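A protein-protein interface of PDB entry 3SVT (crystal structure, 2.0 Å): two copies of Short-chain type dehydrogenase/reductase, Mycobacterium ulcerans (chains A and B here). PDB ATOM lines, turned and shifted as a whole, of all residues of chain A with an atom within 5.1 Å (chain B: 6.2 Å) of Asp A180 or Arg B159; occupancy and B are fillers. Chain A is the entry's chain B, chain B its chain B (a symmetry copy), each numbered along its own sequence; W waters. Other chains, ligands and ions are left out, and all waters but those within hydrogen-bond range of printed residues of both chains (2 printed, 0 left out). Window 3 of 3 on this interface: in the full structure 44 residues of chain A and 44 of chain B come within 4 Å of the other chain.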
ATOM      1  N   MET A 175      13.627  -4.490   2.890  1.00  0.00           N
ATOM      2  CA  MET A 175      13.178  -5.886   2.897  1.00  0.00           C
ATOM      3  C   MET A 175      13.638  -6.594   4.170  1.00  0.00           C
ATOM      4  O   MET A 175      12.845  -7.295   4.846  1.00  0.00           O
ATOM      5  CB  MET A 175      13.713  -6.657   1.684  1.00  0.00           C
ATOM      6  CG  MET A 175      13.251  -6.213   0.286  1.00  0.00           C
ATOM      7  SD  MET A 175      11.489  -6.117  -0.018  1.00  0.00           S
ATOM      8  CE  MET A 175      11.183  -4.385   0.405  1.00  0.00           C
ATOM      9  N   GLN A 176      14.909  -6.407   4.516  1.00  0.00           N
ATOM     10  CA  GLN A 176      15.438  -6.987   5.768  1.00  0.00           C
ATOM     11  C   GLN A 176      14.771  -6.452   7.057  1.00  0.00           C
ATOM     12  O   GLN A 176      14.395  -7.243   7.930  1.00  0.00           O
ATOM     13  CB  GLN A 176      16.955  -6.851   5.811  1.00  0.00           C
ATOM     14  CG  GLN A 176      17.599  -7.722   4.747  1.00  0.00           C
ATOM     15  CD  GLN A 176      19.077  -7.777   4.862  1.00  0.00           C
ATOM     16  OE1 GLN A 176      19.722  -6.740   4.989  1.00  0.00           O
ATOM     17  NE2 GLN A 176      19.635  -8.986   4.823  1.00  0.00           N
ATOM     18  N   LEU A 177      14.570  -5.128   7.140  1.00  0.00           N
ATOM     19  CA  LEU A 177      13.841  -4.531   8.256  1.00  0.00           C
ATOM     20  C   LEU A 177      12.433  -5.123   8.400  1.00  0.00           C
ATOM     21  O   LEU A 177      12.036  -5.549   9.494  1.00  0.00           O
ATOM     22  CB  LEU A 177      13.744  -3.027   8.052  1.00  0.00           C
ATOM     23  CG  LEU A 177      12.987  -2.148   9.052  1.00  0.00           C
ATOM     24  CD1 LEU A 177      13.538  -2.339  10.459  1.00  0.00           C
ATOM     25  CD2 LEU A 177      13.062  -0.670   8.594  1.00  0.00           C
ATOM     26  N   ALA A 178      11.684  -5.151   7.290  1.00  0.00           N
ATOM     27  CA  ALA A 178      10.339  -5.709   7.274  1.00  0.00           C
ATOM     28  C   ALA A 178      10.285  -7.206   7.673  1.00  0.00           C
ATOM     29  O   ALA A 178       9.386  -7.644   8.424  1.00  0.00           O
ATOM     30  CB  ALA A 178       9.685  -5.473   5.905  1.00  0.00           C
ATOM     31  N   ALA A 179      11.228  -7.990   7.160  1.00  0.00           N
ATOM     32  CA  ALA A 179      11.362  -9.395   7.548  1.00  0.00           C
ATOM     33  C   ALA A 179      11.480  -9.485   9.087  1.00  0.00           C
ATOM     34  O   ALA A 179      10.840 -10.315   9.713  1.00  0.00           O
ATOM     35  CB  ALA A 179      12.610 -10.037   6.878  1.00  0.00           C
ATOM     36  N   ASP A 180      12.301  -8.617   9.670  1.00  0.00           N
ATOM     37  CA  ASP A 180      12.543  -8.616  11.130  1.00  0.00           C
ATOM     38  C   ASP A 180      11.225  -8.297  11.877  1.00  0.00           C
ATOM     39  O   ASP A 180      10.855  -8.992  12.822  1.00  0.00           O
ATOM     40  CB  ASP A 180      13.617  -7.592  11.477  1.00  0.00           C
ATOM     41  CG  ASP A 180      14.309  -7.845  12.836  1.00  0.00           C
ATOM     42  OD1 ASP A 180      13.838  -8.660  13.659  1.00  0.00           O
ATOM     43  OD2 ASP A 180      15.377  -7.209  13.066  1.00  0.00           O
ATOM     44  N   GLU A 181      10.531  -7.259  11.407  1.00  0.00           N
ATOM     45  CA  GLU A 181       9.278  -6.805  12.017  1.00  0.00           C
ATOM     46  C   GLU A 181       8.094  -7.746  11.864  1.00  0.00           C
ATOM     47  O   GLU A 181       7.254  -7.825  12.754  1.00  0.00           O
ATOM     48  CB  GLU A 181       8.859  -5.429  11.467  1.00  0.00           C
ATOM     49  CG  GLU A 181       9.494  -4.293  12.223  1.00  0.00           C
ATOM     50  CD  GLU A 181       9.104  -2.919  11.675  1.00  0.00           C
ATOM     51  OE1 GLU A 181       7.947  -2.754  11.260  1.00  0.00           O
ATOM     52  OE2 GLU A 181       9.963  -2.011  11.664  1.00  0.00           O
ATOM     53  N   LEU A 182       8.024  -8.421  10.719  1.00  0.00           N
ATOM     54  CA  LEU A 182       6.832  -9.108  10.305  1.00  0.00           C
ATOM     55  C   LEU A 182       6.952 -10.611  10.429  1.00  0.00           C
ATOM     56  O   LEU A 182       5.972 -11.315  10.179  1.00  0.00           O
ATOM     57  CB  LEU A 182       6.496  -8.730   8.856  1.00  0.00           C
ATOM     58  CG  LEU A 182       6.253  -7.233   8.589  1.00  0.00           C
ATOM     59  CD1 LEU A 182       6.045  -7.018   7.076  1.00  0.00           C
ATOM     60  CD2 LEU A 182       5.080  -6.675   9.432  1.00  0.00           C
ATOM     61  N   GLY A 183       8.134 -11.116  10.790  1.00  0.00           N
ATOM     62  CA  GLY A 183       8.291 -12.562  10.978  1.00  0.00           C
ATOM     63  C   GLY A 183       7.287 -13.158  11.956  1.00  0.00           C
ATOM     64  O   GLY A 183       6.790 -14.273  11.764  1.00  0.00           O
ATOM     65  N   GLY B 106       7.929   3.492  14.721  1.00  0.00           N
ATOM     66  CA  GLY B 106       6.732   2.669  14.708  1.00  0.00           C
ATOM     67  C   GLY B 106       6.768   1.640  13.594  1.00  0.00           C
ATOM     68  O   GLY B 106       7.695   1.619  12.790  1.00  0.00           O
ATOM     69  N   THR B 157      19.431  -4.292  11.441  1.00  0.00           N
ATOM     70  CA  THR B 157      18.009  -3.882  11.471  1.00  0.00           C
ATOM     71  C   THR B 157      17.542  -3.427  12.876  1.00  0.00           C
ATOM     72  O   THR B 157      17.748  -4.135  13.885  1.00  0.00           O
ATOM     73  CB  THR B 157      17.068  -5.019  11.010  1.00  0.00           C
ATOM     74  OG1 THR B 157      17.340  -6.216  11.767  1.00  0.00           O
ATOM     75  CG2 THR B 157      17.232  -5.275   9.464  1.00  0.00           C
ATOM     76  N   HIS B 158      16.948  -2.229  12.907  1.00  0.00           N
ATOM     77  CA  HIS B 158      16.370  -1.645  14.092  1.00  0.00           C
ATOM     78  C   HIS B 158      14.854  -1.700  13.872  1.00  0.00           C
ATOM     79  O   HIS B 158      14.291  -0.834  13.188  1.00  0.00           O
ATOM     80  CB  HIS B 158      16.812  -0.176  14.271  1.00  0.00           C
ATOM     81  CG  HIS B 158      18.220  -0.001  14.756  1.00  0.00           C
ATOM     82  ND1 HIS B 158      19.255  -0.823  14.357  1.00  0.00           N
ATOM     83  CD2 HIS B 158      18.766   0.918  15.593  1.00  0.00           C
ATOM     84  CE1 HIS B 158      20.375  -0.421  14.938  1.00  0.00           C
ATOM     85  NE2 HIS B 158      20.107   0.633  15.691  1.00  0.00           N
ATOM     86  N   ARG B 159      14.210  -2.730  14.422  1.00  0.00           N
ATOM     87  CA  ARG B 159      12.767  -2.824  14.338  1.00  0.00           C
ATOM     88  C   ARG B 159      12.148  -1.474  14.746  1.00  0.00           C
ATOM     89  O   ARG B 159      12.506  -0.901  15.785  1.00  0.00           O
ATOM     90  CB  ARG B 159      12.236  -3.958  15.250  1.00  0.00           C
ATOM     91  CG  ARG B 159      12.343  -5.367  14.663  1.00  0.00           C
ATOM     92  CD  ARG B 159      12.121  -6.461  15.747  1.00  0.00           C
ATOM     93  NE  ARG B 159      13.384  -6.654  16.475  1.00  0.00           N
ATOM     94  CZ  ARG B 159      13.577  -7.463  17.516  1.00  0.00           C
ATOM     95  NH1 ARG B 159      12.575  -8.153  18.025  1.00  0.00           N
ATOM     96  NH2 ARG B 159      14.796  -7.554  18.065  1.00  0.00           N
ATOM     97  N   TRP B 160      11.253  -0.988  13.890  1.00  0.00           N
ATOM     98  CA  TRP B 160      10.374   0.166  14.124  1.00  0.00           C
ATOM     99  C   TRP B 160      11.058   1.515  13.902  1.00  0.00           C
ATOM    100  O   TRP B 160      10.513   2.560  14.262  1.00  0.00           O
ATOM    101  CB  TRP B 160       9.686   0.092  15.483  1.00  0.00           C
ATOM    102  CG  TRP B 160       9.091  -1.269  15.736  1.00  0.00           C
ATOM    103  CD1 TRP B 160       8.052  -1.841  15.075  1.00  0.00           C
ATOM    104  CD2 TRP B 160       9.523  -2.219  16.707  1.00  0.00           C
ATOM    105  NE1 TRP B 160       7.801  -3.099  15.569  1.00  0.00           N
ATOM    106  CE2 TRP B 160       8.679  -3.346  16.592  1.00  0.00           C
ATOM    107  CE3 TRP B 160      10.526  -2.222  17.684  1.00  0.00           C
ATOM    108  CZ2 TRP B 160       8.838  -4.479  17.387  1.00  0.00           C
ATOM    109  CZ3 TRP B 160      10.656  -3.342  18.496  1.00  0.00           C
ATOM    110  CH2 TRP B 160       9.821  -4.457  18.334  1.00  0.00           C
ATOM    111  N   PHE B 161      12.245   1.489  13.292  1.00  0.00           N
ATOM    112  CA  PHE B 161      12.982   2.722  13.023  1.00  0.00           C
ATOM    113  C   PHE B 161      12.705   3.210  11.626  1.00  0.00           C
ATOM    114  O   PHE B 161      13.225   4.251  11.249  1.00  0.00           O
ATOM    115  CB  PHE B 161      14.493   2.555  13.259  1.00  0.00           C
ATOM    116  CG  PHE B 161      14.904   2.735  14.701  1.00  0.00           C
ATOM    117  CD1 PHE B 161      14.334   1.956  15.710  1.00  0.00           C
ATOM    118  CD2 PHE B 161      15.841   3.693  15.054  1.00  0.00           C
ATOM    119  CE1 PHE B 161      14.707   2.125  17.040  1.00  0.00           C
ATOM    120  CE2 PHE B 161      16.233   3.863  16.386  1.00  0.00           C
ATOM    121  CZ  PHE B 161      15.672   3.080  17.370  1.00  0.00           C
ATOM    122  N   GLY B 162      11.903   2.447  10.865  1.00  0.00           N
ATOM    123  CA  GLY B 162      11.408   2.875   9.565  1.00  0.00           C
ATOM    124  C   GLY B 162      12.527   3.374   8.664  1.00  0.00           C
ATOM    125  O   GLY B 162      13.445   2.626   8.325  1.00  0.00           O
ATOM    126  N   ARG B 260      22.927  -7.646  17.886  1.00  0.00           N
ATOM    127  CA  ARG B 260      21.769  -7.181  17.120  1.00  0.00           C
ATOM    128  C   ARG B 260      21.492  -5.702  17.365  1.00  0.00           C
ATOM    129  O   ARG B 260      22.036  -5.089  18.278  1.00  0.00           O
ATOM    130  CB  ARG B 260      20.535  -8.008  17.472  1.00  0.00           C
ATOM    131  CG  ARG B 260      20.179  -8.006  18.933  1.00  0.00           C
ATOM    132  CD  ARG B 260      18.760  -8.465  19.171  1.00  0.00           C
ATOM    133  NE  ARG B 260      18.509  -8.567  20.599  1.00  0.00           N
ATOM    134  CZ  ARG B 260      18.192  -7.539  21.387  1.00  0.00           C
ATOM    135  NH1 ARG B 260      18.051  -6.306  20.901  1.00  0.00           N
ATOM    136  NH2 ARG B 260      17.987  -7.744  22.672  1.00  0.00           N
ATOM    137  N   GLY B 261      20.631  -5.120  16.533  1.00  0.00           N
ATOM    138  CA  GLY B 261      20.105  -3.823  16.835  1.00  0.00           C
ATOM    139  C   GLY B 261      19.261  -3.893  18.103  1.00  0.00           C
ATOM    140  O   GLY B 261      18.879  -4.973  18.536  1.00  0.00           O
ATOM    141  N   PRO B 262      18.935  -2.727  18.683  1.00  0.00           N
ATOM    142  CA  PRO B 262      18.129  -2.664  19.881  1.00  0.00           C
ATOM    143  C   PRO B 262      16.667  -3.053  19.661  1.00  0.00           C
ATOM    144  O   PRO B 262      16.117  -2.940  18.547  1.00  0.00           O
ATOM    145  CB  PRO B 262      18.235  -1.191  20.287  1.00  0.00           C
ATOM    146  CG  PRO B 262      18.317  -0.489  18.985  1.00  0.00           C
ATOM    147  CD  PRO B 262      19.238  -1.384  18.158  1.00  0.00           C
ATOM    148  N   ASP B 263      16.063  -3.516  20.745  1.00  0.00           N
ATOM    149  CA  ASP B 263      14.649  -3.881  20.805  1.00  0.00           C
ATOM    150  C   ASP B 263      13.959  -2.806  21.639  1.00  0.00           C
ATOM    151  O   ASP B 263      14.154  -2.747  22.855  1.00  0.00           O
ATOM    152  CB  ASP B 263      14.543  -5.254  21.469  1.00  0.00           C
ATOM    153  CG  ASP B 263      13.113  -5.722  21.665  1.00  0.00           C
ATOM    154  OD1 ASP B 263      12.134  -5.005  21.322  1.00  0.00           O
ATOM    155  OD2 ASP B 263      12.991  -6.836  22.188  1.00  0.00           O
ATOM    156  N   PHE B 264      13.158  -1.956  20.986  1.00  0.00           N
ATOM    157  CA  PHE B 264      12.491  -0.826  21.657  1.00  0.00           C
ATOM    158  C   PHE B 264      11.094  -1.217  22.158  1.00  0.00           C
ATOM    159  O   PHE B 264      10.278  -0.341  22.463  1.00  0.00           O
ATOM    160  CB  PHE B 264      12.398   0.399  20.740  1.00  0.00           C
ATOM    161  CG  PHE B 264      13.608   1.330  20.801  1.00  0.00           C
ATOM    162  CD1 PHE B 264      14.895   0.862  20.526  1.00  0.00           C
ATOM    163  CD2 PHE B 264      13.437   2.684  21.096  1.00  0.00           C
ATOM    164  CE1 PHE B 264      16.000   1.720  20.597  1.00  0.00           C
ATOM    165  CE2 PHE B 264      14.531   3.579  21.151  1.00  0.00           C
ATOM    166  CZ  PHE B 264      15.824   3.098  20.894  1.00  0.00           C
ATOM    167  N   SER B 265      10.825  -2.523  22.241  1.00  0.00           N
ATOM    168  CA  SER B 265       9.527  -3.047  22.695  1.00  0.00           C
ATOM    169  C   SER B 265       8.998  -2.328  23.909  1.00  0.00           C
ATOM    170  O   SER B 265       7.874  -1.847  23.906  1.00  0.00           O
ATOM    171  CB  SER B 265       9.641  -4.521  23.080  1.00  0.00           C
ATOM    172  OG  SER B 265       9.801  -5.298  21.941  1.00  0.00           O
ATOM    173  N   LEU B 268       7.611   0.972  23.162  1.00  0.00           N
ATOM    174  CA  LEU B 268       6.585   1.049  22.102  1.00  0.00           C
ATOM    175  C   LEU B 268       5.332   0.212  22.378  1.00  0.00           C
ATOM    176  O   LEU B 268       4.218   0.595  21.980  1.00  0.00           O
ATOM    177  CB  LEU B 268       7.186   0.665  20.739  1.00  0.00           C
ATOM    178  CG  LEU B 268       8.369   1.514  20.213  1.00  0.00           C
ATOM    179  CD1 LEU B 268       8.912   0.947  18.890  1.00  0.00           C
ATOM    180  CD2 LEU B 268       7.986   2.996  20.044  1.00  0.00           C
HETATM  181  O   HOH W   1      16.506  -6.914  15.648  1.00  0.00           O
HETATM  182  O   HOH W   2       9.746   0.742  10.966  1.00  0.00           O
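The side-chain carboxylate (OD1) of Asp A180 is in salt-bridge range of the guanidinium group (NE) of Arg B159 (3.5 Å).
OG1 of Thr B157 lies within hydrogen-bond range of OD2 of Asp A180.
The side-chain carboxylate of Glu A181 is in hydrogen-bond range of the backbone NH of Trp B160 (2.8 Å).
The backbone NH (N) of Gly B106 lies within hydrogen-bond range of the backbone carbonyl oxygen (O) of Trp B160 (2.8 Å).
Gln A176 touches Thr B157.
Leu A177 touches Thr B157 (N to CG2, 3.5 Å).
His B158 touches Leu A177.
Arg B159 touches Leu A177.
Leu A177 touches Gly B162 (CD2 to O, 3.3 Å).
Glu A181 touches Arg B159 (OE2 to C, 3.8 Å).
Of chain B, only Thr B157 (2.6 Å) and Arg B159 (3.5 Å) come within 4 Å of Asp A180.
Of the printed residues of chain A, Gly B162 touches Leu A177.
Of the printed residues of chain B, Glu A181 touches Arg B159 (3.8 Å) and Trp B160 (2.8 Å).
Of the printed residues of chain A, Thr B157 touches Gln A176 (3.6 Å), Leu A177 (3.5 Å) and Asp A180 (2.6 Å).
Printed residues of chain A within 4 Å of His B158: Leu A177 (3.2 Å).
Met A175 touches none of the printed residues of chain B.
The nearest printed residue of chain A that does not touch Arg B159 is Leu A182 (6.6 Å).
Of the 9 printed residues of chain A, 4 touch a printed residue of chain B.
Hydrophobic or aromatic side chains of chain A that line the printed part of chain B: Leu A177.
Along chain A the printed residues that touch a printed residue of chain B span positions 176 to 181.
No position is printed for both chains.
Water W2 lies within hydrogen-bond range of the backbone NH of Gly B162, the side-chain carboxylate of Glu A181, the backbone carbonyl oxygen of Gly B106 and the backbone NH of Phe B161.
Water W1 lies within hydrogen-bond range of OD2 of Asp A180 and NH2 of Arg B159.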
